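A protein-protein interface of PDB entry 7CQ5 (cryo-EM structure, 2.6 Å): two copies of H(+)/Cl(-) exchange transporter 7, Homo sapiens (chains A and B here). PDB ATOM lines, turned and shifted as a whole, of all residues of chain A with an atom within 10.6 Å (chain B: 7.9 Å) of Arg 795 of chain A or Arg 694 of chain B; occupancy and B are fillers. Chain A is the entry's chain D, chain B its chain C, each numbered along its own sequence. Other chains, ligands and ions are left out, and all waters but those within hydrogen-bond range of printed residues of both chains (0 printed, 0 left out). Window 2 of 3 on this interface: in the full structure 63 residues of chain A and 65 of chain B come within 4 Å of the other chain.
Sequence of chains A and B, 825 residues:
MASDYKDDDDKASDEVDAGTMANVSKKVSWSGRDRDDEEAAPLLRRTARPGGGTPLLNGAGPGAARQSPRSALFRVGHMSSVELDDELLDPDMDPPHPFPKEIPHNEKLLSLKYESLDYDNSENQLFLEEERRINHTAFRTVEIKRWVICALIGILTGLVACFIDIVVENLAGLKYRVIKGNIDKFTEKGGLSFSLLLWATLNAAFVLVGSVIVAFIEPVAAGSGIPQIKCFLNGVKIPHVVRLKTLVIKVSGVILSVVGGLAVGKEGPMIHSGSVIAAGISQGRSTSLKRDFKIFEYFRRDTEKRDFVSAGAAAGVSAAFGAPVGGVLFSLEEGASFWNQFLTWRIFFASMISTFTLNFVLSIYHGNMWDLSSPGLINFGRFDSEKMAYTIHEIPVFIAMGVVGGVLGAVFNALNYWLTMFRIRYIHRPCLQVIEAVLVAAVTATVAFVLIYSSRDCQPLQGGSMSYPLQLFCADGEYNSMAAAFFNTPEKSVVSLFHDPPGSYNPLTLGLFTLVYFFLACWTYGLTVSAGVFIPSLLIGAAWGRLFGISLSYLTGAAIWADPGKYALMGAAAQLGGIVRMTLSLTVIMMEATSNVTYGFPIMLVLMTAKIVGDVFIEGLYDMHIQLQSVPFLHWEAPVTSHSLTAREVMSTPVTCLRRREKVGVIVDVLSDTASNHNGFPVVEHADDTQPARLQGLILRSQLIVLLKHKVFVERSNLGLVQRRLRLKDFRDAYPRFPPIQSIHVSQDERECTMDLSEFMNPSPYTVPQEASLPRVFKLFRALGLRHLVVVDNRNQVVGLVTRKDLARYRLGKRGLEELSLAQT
Of the 18 printed residues of chain B, 5 touch a printed residue of chain A. Printed residues of chain B that touch a printed residue of chain A: Arg 694, Gln 696, Asn 794, Arg 795 and Asn 796. Among the printed residues, no Asp or Glu carboxylate lies within 4 Å of a Lys or Arg side-chain nitrogen of the other chain.
Gln 770 of chain A touches none of the printed residues of chain B. Of chain B, only Arg 694 comes within 4 Å of Arg 795 of chain A. Of the printed residues of chain B, Asn 796 of chain A touches Asn 794 and Arg 795. Leu 658 of chain B touches none of the printed residues of chain A. No residue of chain A comes within 4 Å of Glu 685 of chain B. No residue of chain A comes within 4 Å of Leu 695 of chain B. Printed residues of chain A within 4 Å of Asn 794 of chain B: Leu 695 (3.5 Å), Gln 696 (3.1 Å) and Asn 796 (2.6 Å). Asn 796 of chain B touches just these residues of chain A: Asp 793 (3.7 Å) and Asn 794 (3.2 Å). No residue of chain A comes within 4 Å of Gln 797 of chain B. The nearest residue of chain B that does not touch Arg 795 of chain A is Asn 796 of chain B (4.5 Å). The nearest printed residue of chain B that does not touch Leu 695 of chain A is Arg 795 of chain B (6.8 Å).
Arg 694 of chain A touches Arg 795 of chain B. O of Leu 695 of chain A touches OD1 of Asn 794 of chain B (3.5 Å). Asp 793 of chain A touches Asn 796 of chain B (O to OD1, 3.7 Å). Asn 794 of chain A touches Arg 694 of chain B (O to CD, 3.3 Å). Gln 696 of chain B touches Asn 794 of chain A. Arg 795 of chain A touches Arg 694 of chain B (CD to NH1, 3.7 Å). Arg 795 of chain B touches Asn 796 of chain A (O to ND2, 3.9 Å).
The side-chain amide nitrogen of Gln 696 of chain A is in hydrogen-bond range of the side-chain amide oxygen of Asn 794 of chain B (3.1 Å). O of Asn 794 of chain B lies within hydrogen-bond range of ND2 of Asn 796 of chain A (2.6 Å).
O of Arg 694 of chain B is in hydrogen-bond range of N of Glu 685 of chain B (3.2 Å). NE2 of Gln 696 of chain B sits close to OE2 of Glu 685 of chain B. N of Gln 696 of chain B lies within hydrogen-bond range of O of Val 683 of chain B (2.9 Å). The guanidinium group (NH1) of Arg 795 of chain B sits at hydrogen-bond distance from the side-chain amide oxygen (OE1) of Gln 797 of chain B.
Arg 694 of chain A touches Arg 795 of chain B, and with the chains exchanged Arg 795 of chain A touches Arg 694 of chain B. Asn 796 of chain A touches Arg 795 of chain B, but with the chains exchanged Arg 795 of chain A does not touch Asn 796 of chain B (4.5 Å). Of the 10 pairs that touch across the chains among the printed residues, 6 have their exchanged pair printed and touching as well.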
ATOM      1  N   VAL A 684     -13.240  37.549 -17.757  1.00  0.00           N
ATOM      2  CA  VAL A 684     -14.495  37.412 -17.048  1.00  0.00           C
ATOM      3  C   VAL A 684     -15.674  37.986 -17.824  1.00  0.00           C
ATOM      4  O   VAL A 684     -15.519  38.899 -18.627  1.00  0.00           O
ATOM      5  CB  VAL A 684     -14.398  38.055 -15.646  1.00  0.00           C
ATOM      6  CG1 VAL A 684     -13.358  37.347 -14.812  1.00  0.00           C
ATOM      7  CG2 VAL A 684     -14.078  39.533 -15.742  1.00  0.00           C
ATOM      8  N   ALA A 693     -18.994  39.376 -12.585  1.00  0.00           N
ATOM      9  CA  ALA A 693     -17.860  38.958 -13.403  1.00  0.00           C
ATOM     10  C   ALA A 693     -17.649  37.452 -13.306  1.00  0.00           C
ATOM     11  O   ALA A 693     -16.862  36.975 -12.497  1.00  0.00           O
ATOM     12  CB  ALA A 693     -16.605  39.701 -12.986  1.00  0.00           C
ATOM     13  N   ARG A 694     -18.369  36.709 -14.138  1.00  0.00           N
ATOM     14  CA  ARG A 694     -18.267  35.260 -14.146  1.00  0.00           C
ATOM     15  C   ARG A 694     -17.055  34.829 -14.950  1.00  0.00           C
ATOM     16  O   ARG A 694     -16.780  35.387 -16.011  1.00  0.00           O
ATOM     17  CB  ARG A 694     -19.518  34.638 -14.758  1.00  0.00           C
ATOM     18  CG  ARG A 694     -20.784  34.880 -13.991  1.00  0.00           C
ATOM     19  CD  ARG A 694     -21.940  34.240 -14.716  1.00  0.00           C
ATOM     20  NE  ARG A 694     -23.208  34.504 -14.054  1.00  0.00           N
ATOM     21  CZ  ARG A 694     -23.999  35.528 -14.346  1.00  0.00           C
ATOM     22  NH1 ARG A 694     -23.650  36.384 -15.294  1.00  0.00           N
ATOM     23  NH2 ARG A 694     -25.140  35.696 -13.693  1.00  0.00           N
ATOM     24  N   LEU A 695     -16.355  33.812 -14.455  1.00  0.00           N
ATOM     25  CA  LEU A 695     -15.172  33.298 -15.130  1.00  0.00           C
ATOM     26  C   LEU A 695     -15.531  32.663 -16.467  1.00  0.00           C
ATOM     27  O   LEU A 695     -16.373  31.764 -16.539  1.00  0.00           O
ATOM     28  CB  LEU A 695     -14.473  32.272 -14.246  1.00  0.00           C
ATOM     29  CG  LEU A 695     -13.178  31.685 -14.798  1.00  0.00           C
ATOM     30  CD1 LEU A 695     -12.112  32.746 -14.921  1.00  0.00           C
ATOM     31  CD2 LEU A 695     -12.714  30.564 -13.925  1.00  0.00           C
ATOM     32  N   GLN A 696     -14.890  33.145 -17.527  1.00  0.00           N
ATOM     33  CA  GLN A 696     -15.044  32.589 -18.860  1.00  0.00           C
ATOM     34  C   GLN A 696     -13.838  31.785 -19.304  1.00  0.00           C
ATOM     35  O   GLN A 696     -13.985  30.854 -20.093  1.00  0.00           O
ATOM     36  CB  GLN A 696     -15.288  33.712 -19.873  1.00  0.00           C
ATOM     37  CG  GLN A 696     -16.470  34.582 -19.524  1.00  0.00           C
ATOM     38  CD  GLN A 696     -17.765  33.820 -19.542  1.00  0.00           C
ATOM     39  OE1 GLN A 696     -17.999  32.991 -20.420  1.00  0.00           O
ATOM     40  NE2 GLN A 696     -18.614  34.075 -18.559  1.00  0.00           N
ATOM     41  N   THR A 767     -10.212  25.249 -11.575  1.00  0.00           N
ATOM     42  CA  THR A 767     -10.692  26.073 -10.480  1.00  0.00           C
ATOM     43  C   THR A 767     -10.775  25.250  -9.208  1.00  0.00           C
ATOM     44  O   THR A 767     -10.950  24.032  -9.243  1.00  0.00           O
ATOM     45  CB  THR A 767     -12.081  26.679 -10.747  1.00  0.00           C
ATOM     46  OG1 THR A 767     -13.045  25.629 -10.879  1.00  0.00           O
ATOM     47  CG2 THR A 767     -12.083  27.496 -11.998  1.00  0.00           C
ATOM     48  N   VAL A 768     -10.632  25.933  -8.080  1.00  0.00           N
ATOM     49  CA  VAL A 768     -10.946  25.353  -6.781  1.00  0.00           C
ATOM     50  C   VAL A 768     -11.966  26.259  -6.108  1.00  0.00           C
ATOM     51  O   VAL A 768     -12.013  27.462  -6.399  1.00  0.00           O
ATOM     52  CB  VAL A 768      -9.691  25.165  -5.913  1.00  0.00           C
ATOM     53  CG1 VAL A 768      -8.777  24.117  -6.522  1.00  0.00           C
ATOM     54  CG2 VAL A 768      -8.955  26.483  -5.737  1.00  0.00           C
ATOM     55  N   PRO A 769     -12.826  25.727  -5.249  1.00  0.00           N
ATOM     56  CA  PRO A 769     -13.684  26.595  -4.445  1.00  0.00           C
ATOM     57  C   PRO A 769     -12.879  27.323  -3.383  1.00  0.00           C
ATOM     58  O   PRO A 769     -11.744  26.969  -3.061  1.00  0.00           O
ATOM     59  CB  PRO A 769     -14.682  25.622  -3.813  1.00  0.00           C
ATOM     60  CG  PRO A 769     -14.666  24.446  -4.695  1.00  0.00           C
ATOM     61  CD  PRO A 769     -13.258  24.325  -5.173  1.00  0.00           C
ATOM     62  N   GLN A 770     -13.512  28.350  -2.821  1.00  0.00           N
ATOM     63  CA  GLN A 770     -12.876  29.189  -1.819  1.00  0.00           C
ATOM     64  C   GLN A 770     -12.661  28.447  -0.503  1.00  0.00           C
ATOM     65  O   GLN A 770     -11.801  28.839   0.291  1.00  0.00           O
ATOM     66  CB  GLN A 770     -13.740  30.432  -1.621  1.00  0.00           C
ATOM     67  CG  GLN A 770     -13.109  31.566  -0.880  1.00  0.00           C
ATOM     68  CD  GLN A 770     -14.014  32.769  -0.823  1.00  0.00           C
ATOM     69  OE1 GLN A 770     -15.152  32.723  -1.284  1.00  0.00           O
ATOM     70  NE2 GLN A 770     -13.509  33.863  -0.268  1.00  0.00           N
ATOM     71  N   GLU A 771     -13.401  27.365  -0.280  1.00  0.00           N
ATOM     72  CA  GLU A 771     -13.347  26.585   0.943  1.00  0.00           C
ATOM     73  C   GLU A 771     -12.513  25.318   0.804  1.00  0.00           C
ATOM     74  O   GLU A 771     -12.472  24.518   1.743  1.00  0.00           O
ATOM     75  CB  GLU A 771     -14.766  26.211   1.385  1.00  0.00           C
ATOM     76  CG  GLU A 771     -15.655  27.389   1.763  1.00  0.00           C
ATOM     77  CD  GLU A 771     -16.378  28.002   0.576  1.00  0.00           C
ATOM     78  OE1 GLU A 771     -16.250  27.471  -0.546  1.00  0.00           O
ATOM     79  OE2 GLU A 771     -17.071  29.023   0.762  1.00  0.00           O
ATOM     80  N   VAL A 791      -9.418  30.769  -8.061  1.00  0.00           N
ATOM     81  CA  VAL A 791     -10.310  30.492  -6.944  1.00  0.00           C
ATOM     82  C   VAL A 791     -11.618  31.231  -7.188  1.00  0.00           C
ATOM     83  O   VAL A 791     -11.615  32.436  -7.464  1.00  0.00           O
ATOM     84  CB  VAL A 791      -9.680  30.920  -5.608  1.00  0.00           C
ATOM     85  CG1 VAL A 791     -10.602  30.594  -4.457  1.00  0.00           C
ATOM     86  CG2 VAL A 791      -8.321  30.288  -5.419  1.00  0.00           C
ATOM     87  N   VAL A 792     -12.738  30.512  -7.085  1.00  0.00           N
ATOM     88  CA  VAL A 792     -14.053  31.041  -7.422  1.00  0.00           C
ATOM     89  C   VAL A 792     -14.989  30.928  -6.223  1.00  0.00           C
ATOM     90  O   VAL A 792     -14.759  30.165  -5.284  1.00  0.00           O
ATOM     91  CB  VAL A 792     -14.665  30.324  -8.645  1.00  0.00           C
ATOM     92  CG1 VAL A 792     -13.875  30.626  -9.892  1.00  0.00           C
ATOM     93  CG2 VAL A 792     -14.694  28.829  -8.406  1.00  0.00           C
ATOM     94  N   ASP A 793     -16.058  31.723  -6.272  1.00  0.00           N
ATOM     95  CA  ASP A 793     -17.210  31.604  -5.390  1.00  0.00           C
ATOM     96  C   ASP A 793     -18.089  30.423  -5.794  1.00  0.00           C
ATOM     97  O   ASP A 793     -17.795  29.676  -6.730  1.00  0.00           O
ATOM     98  CB  ASP A 793     -18.042  32.881  -5.428  1.00  0.00           C
ATOM     99  CG  ASP A 793     -17.450  33.986  -4.615  1.00  0.00           C
ATOM    100  OD1 ASP A 793     -16.802  33.682  -3.593  1.00  0.00           O
ATOM    101  OD2 ASP A 793     -17.643  35.161  -4.988  1.00  0.00           O
ATOM    102  N   ASN A 794     -19.213  30.269  -5.093  1.00  0.00           N
ATOM    103  CA  ASN A 794     -20.304  29.424  -5.555  1.00  0.00           C
ATOM    104  C   ASN A 794     -21.262  30.168  -6.480  1.00  0.00           C
ATOM    105  O   ASN A 794     -22.335  29.651  -6.791  1.00  0.00           O
ATOM    106  CB  ASN A 794     -21.065  28.821  -4.368  1.00  0.00           C
ATOM    107  CG  ASN A 794     -21.571  29.867  -3.391  1.00  0.00           C
ATOM    108  OD1 ASN A 794     -21.366  31.066  -3.572  1.00  0.00           O
ATOM    109  ND2 ASN A 794     -22.248  29.410  -2.349  1.00  0.00           N
ATOM    110  N   ARG A 795     -20.908  31.382  -6.874  1.00  0.00           N
ATOM    111  CA  ARG A 795     -21.577  32.164  -7.898  1.00  0.00           C
ATOM    112  C   ARG A 795     -20.757  32.160  -9.189  1.00  0.00           C
ATOM    113  O   ARG A 795     -21.146  32.795 -10.174  1.00  0.00           O
ATOM    114  CB  ARG A 795     -21.803  33.582  -7.329  1.00  0.00           C
ATOM    115  CG  ARG A 795     -22.632  34.621  -8.088  1.00  0.00           C
ATOM    116  CD  ARG A 795     -24.100  34.282  -8.211  1.00  0.00           C
ATOM    117  NE  ARG A 795     -24.815  35.372  -8.876  1.00  0.00           N
ATOM    118  CZ  ARG A 795     -26.050  35.288  -9.362  1.00  0.00           C
ATOM    119  NH1 ARG A 795     -26.725  34.152  -9.278  1.00  0.00           N
ATOM    120  NH2 ARG A 795     -26.607  36.341  -9.948  1.00  0.00           N
ATOM    121  N   ASN A 796     -19.666  31.378  -9.204  1.00  0.00           N
ATOM    122  CA  ASN A 796     -18.620  31.363 -10.240  1.00  0.00           C
ATOM    123  C   ASN A 796     -18.020  32.758 -10.432  1.00  0.00           C
ATOM    124  O   ASN A 796     -17.702  33.181 -11.543  1.00  0.00           O
ATOM    125  CB  ASN A 796     -19.130  30.771 -11.561  1.00  0.00           C
ATOM    126  CG  ASN A 796     -18.005  30.288 -12.465  1.00  0.00           C
ATOM    127  OD1 ASN A 796     -16.834  30.358 -12.108  1.00  0.00           O
ATOM    128  ND2 ASN A 796     -18.361  29.811 -13.646  1.00  0.00           N
ATOM    129  N   GLN A 797     -17.858  33.474  -9.327  1.00  0.00           N
ATOM    130  CA  GLN A 797     -17.283  34.811  -9.299  1.00  0.00           C
ATOM    131  C   GLN A 797     -15.813  34.699  -8.914  1.00  0.00           C
ATOM    132  O   GLN A 797     -15.484  34.045  -7.922  1.00  0.00           O
ATOM    133  CB  GLN A 797     -18.051  35.659  -8.287  1.00  0.00           C
ATOM    134  CG  GLN A 797     -17.635  37.101  -8.112  1.00  0.00           C
ATOM    135  CD  GLN A 797     -17.907  37.948  -9.326  1.00  0.00           C
ATOM    136  OE1 GLN A 797     -16.984  38.432  -9.977  1.00  0.00           O
ATOM    137  NE2 GLN A 797     -19.184  38.111  -9.660  1.00  0.00           N
ATOM    138  N   VAL A 798     -14.933  35.307  -9.710  1.00  0.00           N
ATOM    139  CA  VAL A 798     -13.491  35.178  -9.501  1.00  0.00           C
ATOM    140  C   VAL A 798     -13.081  35.939  -8.247  1.00  0.00           C
ATOM    141  O   VAL A 798     -13.217  37.165  -8.174  1.00  0.00           O
ATOM    142  CB  VAL A 798     -12.710  35.681 -10.721  1.00  0.00           C
ATOM    143  CG1 VAL A 798     -11.211  35.684 -10.435  1.00  0.00           C
ATOM    144  CG2 VAL A 798     -13.014  34.832 -11.934  1.00  0.00           C
ATOM    145  N   VAL A 799     -12.583  35.209  -7.251  1.00  0.00           N
ATOM    146  CA  VAL A 799     -12.040  35.793  -6.023  1.00  0.00           C
ATOM    147  C   VAL A 799     -10.748  35.048  -5.686  1.00  0.00           C
ATOM    148  O   VAL A 799     -10.763  33.991  -5.052  1.00  0.00           O
ATOM    149  CB  VAL A 799     -13.043  35.756  -4.861  1.00  0.00           C
ATOM    150  CG1 VAL A 799     -14.006  36.913  -4.962  1.00  0.00           C
ATOM    151  CG2 VAL A 799     -13.889  34.500  -4.914  1.00  0.00           C
ATOM    152  N   CYS B 657     -30.826  15.980  -7.669  1.00  0.00           N
ATOM    153  CA  CYS B 657     -30.092  16.668  -6.623  1.00  0.00           C
ATOM    154  C   CYS B 657     -30.888  16.658  -5.327  1.00  0.00           C
ATOM    155  O   CYS B 657     -32.038  16.220  -5.270  1.00  0.00           O
ATOM    156  CB  CYS B 657     -29.781  18.109  -7.040  1.00  0.00           C
ATOM    157  SG  CYS B 657     -28.685  18.264  -8.451  1.00  0.00           S
ATOM    158  N   LEU B 658     -30.245  17.152  -4.278  1.00  0.00           N
ATOM    159  CA  LEU B 658     -30.862  17.338  -2.979  1.00  0.00           C
ATOM    160  C   LEU B 658     -30.575  18.767  -2.548  1.00  0.00           C
ATOM    161  O   LEU B 658     -29.636  19.392  -3.031  1.00  0.00           O
ATOM    162  CB  LEU B 658     -30.305  16.346  -1.950  1.00  0.00           C
ATOM    163  CG  LEU B 658     -30.385  14.849  -2.278  1.00  0.00           C
ATOM    164  CD1 LEU B 658     -29.689  14.040  -1.209  1.00  0.00           C
ATOM    165  CD2 LEU B 658     -31.806  14.356  -2.495  1.00  0.00           C
ATOM    166  N   ARG B 660     -29.666  21.574   0.623  1.00  0.00           N
ATOM    167  CA  ARG B 660     -28.844  21.547   1.833  1.00  0.00           C
ATOM    168  C   ARG B 660     -29.671  21.196   3.054  1.00  0.00           C
ATOM    169  O   ARG B 660     -29.220  20.456   3.933  1.00  0.00           O
ATOM    170  CB  ARG B 660     -28.174  22.895   2.077  1.00  0.00           C
ATOM    171  CG  ARG B 660     -27.069  23.285   1.149  1.00  0.00           C
ATOM    172  CD  ARG B 660     -26.594  24.681   1.517  1.00  0.00           C
ATOM    173  NE  ARG B 660     -25.903  24.739   2.797  1.00  0.00           N
ATOM    174  CZ  ARG B 660     -24.581  24.717   2.931  1.00  0.00           C
ATOM    175  NH1 ARG B 660     -23.803  24.672   1.862  1.00  0.00           N
ATOM    176  NH2 ARG B 660     -24.033  24.766   4.137  1.00  0.00           N
ATOM    177  N   PRO B 682     -25.313  15.412  -5.938  1.00  0.00           N
ATOM    178  CA  PRO B 682     -24.876  16.778  -5.650  1.00  0.00           C
ATOM    179  C   PRO B 682     -25.942  17.518  -4.871  1.00  0.00           C
ATOM    180  O   PRO B 682     -27.132  17.421  -5.168  1.00  0.00           O
ATOM    181  CB  PRO B 682     -24.658  17.385  -7.038  1.00  0.00           C
ATOM    182  CG  PRO B 682     -25.487  16.584  -7.937  1.00  0.00           C
ATOM    183  CD  PRO B 682     -25.509  15.193  -7.377  1.00  0.00           C
ATOM    184  N   VAL B 683     -25.508  18.237  -3.848  1.00  0.00           N
ATOM    185  CA  VAL B 683     -26.413  18.984  -2.988  1.00  0.00           C
ATOM    186  C   VAL B 683     -26.359  20.459  -3.374  1.00  0.00           C
ATOM    187  O   VAL B 683     -25.277  21.031  -3.549  1.00  0.00           O
ATOM    188  CB  VAL B 683     -26.108  18.724  -1.500  1.00  0.00           C
ATOM    189  CG1 VAL B 683     -24.667  18.858  -1.206  1.00  0.00           C
ATOM    190  CG2 VAL B 683     -26.870  19.669  -0.626  1.00  0.00           C
ATOM    191  N   VAL B 684     -27.537  21.052  -3.588  1.00  0.00           N
ATOM    192  CA  VAL B 684     -27.685  22.338  -4.263  1.00  0.00           C
ATOM    193  C   VAL B 684     -28.514  23.295  -3.422  1.00  0.00           C
ATOM    194  O   VAL B 684     -28.893  22.980  -2.290  1.00  0.00           O
ATOM    195  CB  VAL B 684     -28.334  22.167  -5.649  1.00  0.00           C
ATOM    196  CG1 VAL B 684     -27.479  21.297  -6.545  1.00  0.00           C
ATOM    197  CG2 VAL B 684     -29.731  21.583  -5.517  1.00  0.00           C
ATOM    198  N   GLU B 685     -28.793  24.472  -3.969  1.00  0.00           N
ATOM    199  CA  GLU B 685     -29.744  25.392  -3.364  1.00  0.00           C
ATOM    200  C   GLU B 685     -31.144  25.198  -3.937  1.00  0.00           C
ATOM    201  O   GLU B 685     -31.810  26.163  -4.315  1.00  0.00           O
ATOM    202  CB  GLU B 685     -29.309  26.835  -3.568  1.00  0.00           C
ATOM    203  CG  GLU B 685     -28.041  27.211  -2.855  1.00  0.00           C
ATOM    204  CD  GLU B 685     -28.152  27.165  -1.340  1.00  0.00           C
ATOM    205  OE1 GLU B 685     -29.258  27.351  -0.793  1.00  0.00           O
ATOM    206  OE2 GLU B 685     -27.111  26.986  -0.687  1.00  0.00           O
ATOM    207  N   ALA B 693     -30.286  26.715  -7.969  1.00  0.00           N
ATOM    208  CA  ALA B 693     -29.753  25.362  -8.076  1.00  0.00           C
ATOM    209  C   ALA B 693     -28.235  25.376  -8.215  1.00  0.00           C
ATOM    210  O   ALA B 693     -27.661  24.567  -8.943  1.00  0.00           O
ATOM    211  CB  ALA B 693     -30.383  24.639  -9.250  1.00  0.00           C
ATOM    212  N   ARG B 694     -27.593  26.302  -7.511  1.00  0.00           N
ATOM    213  CA  ARG B 694     -26.140  26.379  -7.515  1.00  0.00           C
ATOM    214  C   ARG B 694     -25.542  25.236  -6.711  1.00  0.00           C
ATOM    215  O   ARG B 694     -26.062  24.861  -5.660  1.00  0.00           O
ATOM    216  CB  ARG B 694     -25.671  27.710  -6.940  1.00  0.00           C
ATOM    217  CG  ARG B 694     -26.029  28.908  -7.781  1.00  0.00           C
ATOM    218  CD  ARG B 694     -25.583  30.182  -7.111  1.00  0.00           C
ATOM    219  NE  ARG B 694     -26.287  30.371  -5.851  1.00  0.00           N
ATOM    220  CZ  ARG B 694     -26.033  31.345  -4.990  1.00  0.00           C
ATOM    221  NH1 ARG B 694     -25.091  32.237  -5.253  1.00  0.00           N
ATOM    222  NH2 ARG B 694     -26.725  31.429  -3.865  1.00  0.00           N
ATOM    223  N   LEU B 695     -24.436  24.689  -7.212  1.00  0.00           N
ATOM    224  CA  LEU B 695     -23.771  23.567  -6.564  1.00  0.00           C
ATOM    225  C   LEU B 695     -23.159  23.979  -5.233  1.00  0.00           C
ATOM    226  O   LEU B 695     -22.435  24.973  -5.148  1.00  0.00           O
ATOM    227  CB  LEU B 695     -22.683  23.001  -7.473  1.00  0.00           C
ATOM    228  CG  LEU B 695     -21.925  21.801  -6.907  1.00  0.00           C
ATOM    229  CD1 LEU B 695     -22.834  20.607  -6.797  1.00  0.00           C
ATOM    230  CD2 LEU B 695     -20.711  21.494  -7.742  1.00  0.00           C
ATOM    231  N   GLN B 696     -23.447  23.201  -4.194  1.00  0.00           N
ATOM    232  CA  GLN B 696     -22.879  23.404  -2.871  1.00  0.00           C
ATOM    233  C   GLN B 696     -21.933  22.290  -2.461  1.00  0.00           C
ATOM    234  O   GLN B 696     -20.955  22.556  -1.763  1.00  0.00           O
ATOM    235  CB  GLN B 696     -23.996  23.524  -1.827  1.00  0.00           C
ATOM    236  CG  GLN B 696     -24.997  24.623  -2.118  1.00  0.00           C
ATOM    237  CD  GLN B 696     -24.407  26.002  -1.991  1.00  0.00           C
ATOM    238  OE1 GLN B 696     -23.677  26.291  -1.048  1.00  0.00           O
ATOM    239  NE2 GLN B 696     -24.702  26.858  -2.953  1.00  0.00           N
ATOM    240  N   GLY B 697     -22.187  21.063  -2.892  1.00  0.00           N
ATOM    241  CA  GLY B 697     -21.300  19.965  -2.567  1.00  0.00           C
ATOM    242  C   GLY B 697     -21.792  18.661  -3.148  1.00  0.00           C
ATOM    243  O   GLY B 697     -22.563  18.649  -4.107  1.00  0.00           O
ATOM    244  N   VAL B 792     -21.000  21.548 -15.012  1.00  0.00           N
ATOM    245  CA  VAL B 792     -21.557  22.776 -14.476  1.00  0.00           C
ATOM    246  C   VAL B 792     -21.735  23.791 -15.605  1.00  0.00           C
ATOM    247  O   VAL B 792     -21.240  23.616 -16.717  1.00  0.00           O
ATOM    248  CB  VAL B 792     -20.671  23.333 -13.340  1.00  0.00           C
ATOM    249  CG1 VAL B 792     -19.510  24.183 -13.873  1.00  0.00           C
ATOM    250  CG2 VAL B 792     -21.485  23.994 -12.259  1.00  0.00           C
ATOM    251  N   ASN B 794     -22.154  28.064 -17.025  1.00  0.00           N
ATOM    252  CA  ASN B 794     -21.343  29.270 -16.907  1.00  0.00           C
ATOM    253  C   ASN B 794     -21.489  29.874 -15.517  1.00  0.00           C
ATOM    254  O   ASN B 794     -20.538  30.452 -14.980  1.00  0.00           O
ATOM    255  CB  ASN B 794     -21.758  30.272 -17.982  1.00  0.00           C
ATOM    256  CG  ASN B 794     -20.763  31.384 -18.171  1.00  0.00           C
ATOM    257  OD1 ASN B 794     -19.707  31.412 -17.546  1.00  0.00           O
ATOM    258  ND2 ASN B 794     -21.102  32.324 -19.040  1.00  0.00           N
ATOM    259  N   ARG B 795     -22.665  29.722 -14.913  1.00  0.00           N
ATOM    260  CA  ARG B 795     -22.855  29.930 -13.485  1.00  0.00           C
ATOM    261  C   ARG B 795     -22.344  28.692 -12.747  1.00  0.00           C
ATOM    262  O   ARG B 795     -21.692  27.816 -13.316  1.00  0.00           O
ATOM    263  CB  ARG B 795     -24.324  30.205 -13.172  1.00  0.00           C
ATOM    264  CG  ARG B 795     -24.819  31.613 -13.459  1.00  0.00           C
ATOM    265  CD  ARG B 795     -25.259  31.806 -14.902  1.00  0.00           C
ATOM    266  NE  ARG B 795     -26.330  30.895 -15.287  1.00  0.00           N
ATOM    267  CZ  ARG B 795     -27.625  31.146 -15.119  1.00  0.00           C
ATOM    268  NH1 ARG B 795     -28.529  30.254 -15.502  1.00  0.00           N
ATOM    269  NH2 ARG B 795     -28.020  32.289 -14.577  1.00  0.00           N
ATOM    270  N   ASN B 796     -22.646  28.576 -11.462  1.00  0.00           N
ATOM    271  CA  ASN B 796     -22.270  27.374 -10.724  1.00  0.00           C
ATOM    272  C   ASN B 796     -23.445  26.412 -10.630  1.00  0.00           C
ATOM    273  O   ASN B 796     -23.637  25.743  -9.614  1.00  0.00           O
ATOM    274  CB  ASN B 796     -21.748  27.742  -9.340  1.00  0.00           C
ATOM    275  CG  ASN B 796     -20.771  26.721  -8.779  1.00  0.00           C
ATOM    276  OD1 ASN B 796     -20.117  26.974  -7.776  1.00  0.00           O
ATOM    277  ND2 ASN B 796     -20.641  25.587  -9.439  1.00  0.00           N
ATOM    278  N   GLN B 797     -24.250  26.329 -11.682  1.00  0.00           N
ATOM    279  CA  GLN B 797     -25.455  25.515 -11.695  1.00  0.00           C
ATOM    280  C   GLN B 797     -25.172  24.153 -12.315  1.00  0.00           C
ATOM    281  O   GLN B 797     -24.600  24.067 -13.404  1.00  0.00           O
ATOM    282  CB  GLN B 797     -26.573  26.234 -12.449  1.00  0.00           C
ATOM    283  CG  GLN B 797     -27.064  27.458 -11.701  1.00  0.00           C
ATOM    284  CD  GLN B 797     -28.116  28.236 -12.448  1.00  0.00           C
ATOM    285  OE1 GLN B 797     -28.437  27.931 -13.594  1.00  0.00           O
ATOM    286  NE2 GLN B 797     -28.667  29.251 -11.797  1.00  0.00           N
ATOM    287  N   VAL B 798     -25.582  23.096 -11.618  1.00  0.00           N
ATOM    288  CA  VAL B 798     -25.263  21.732 -12.029  1.00  0.00           C
ATOM    289  C   VAL B 798     -26.115  21.338 -13.234  1.00  0.00           C
ATOM    290  O   VAL B 798     -27.348  21.415 -13.209  1.00  0.00           O
ATOM    291  CB  VAL B 798     -25.413  20.758 -10.844  1.00  0.00           C
ATOM    292  CG1 VAL B 798     -26.710  20.959 -10.118  1.00  0.00           C
ATOM    293  CG2 VAL B 798     -25.322  19.317 -11.314  1.00  0.00           C
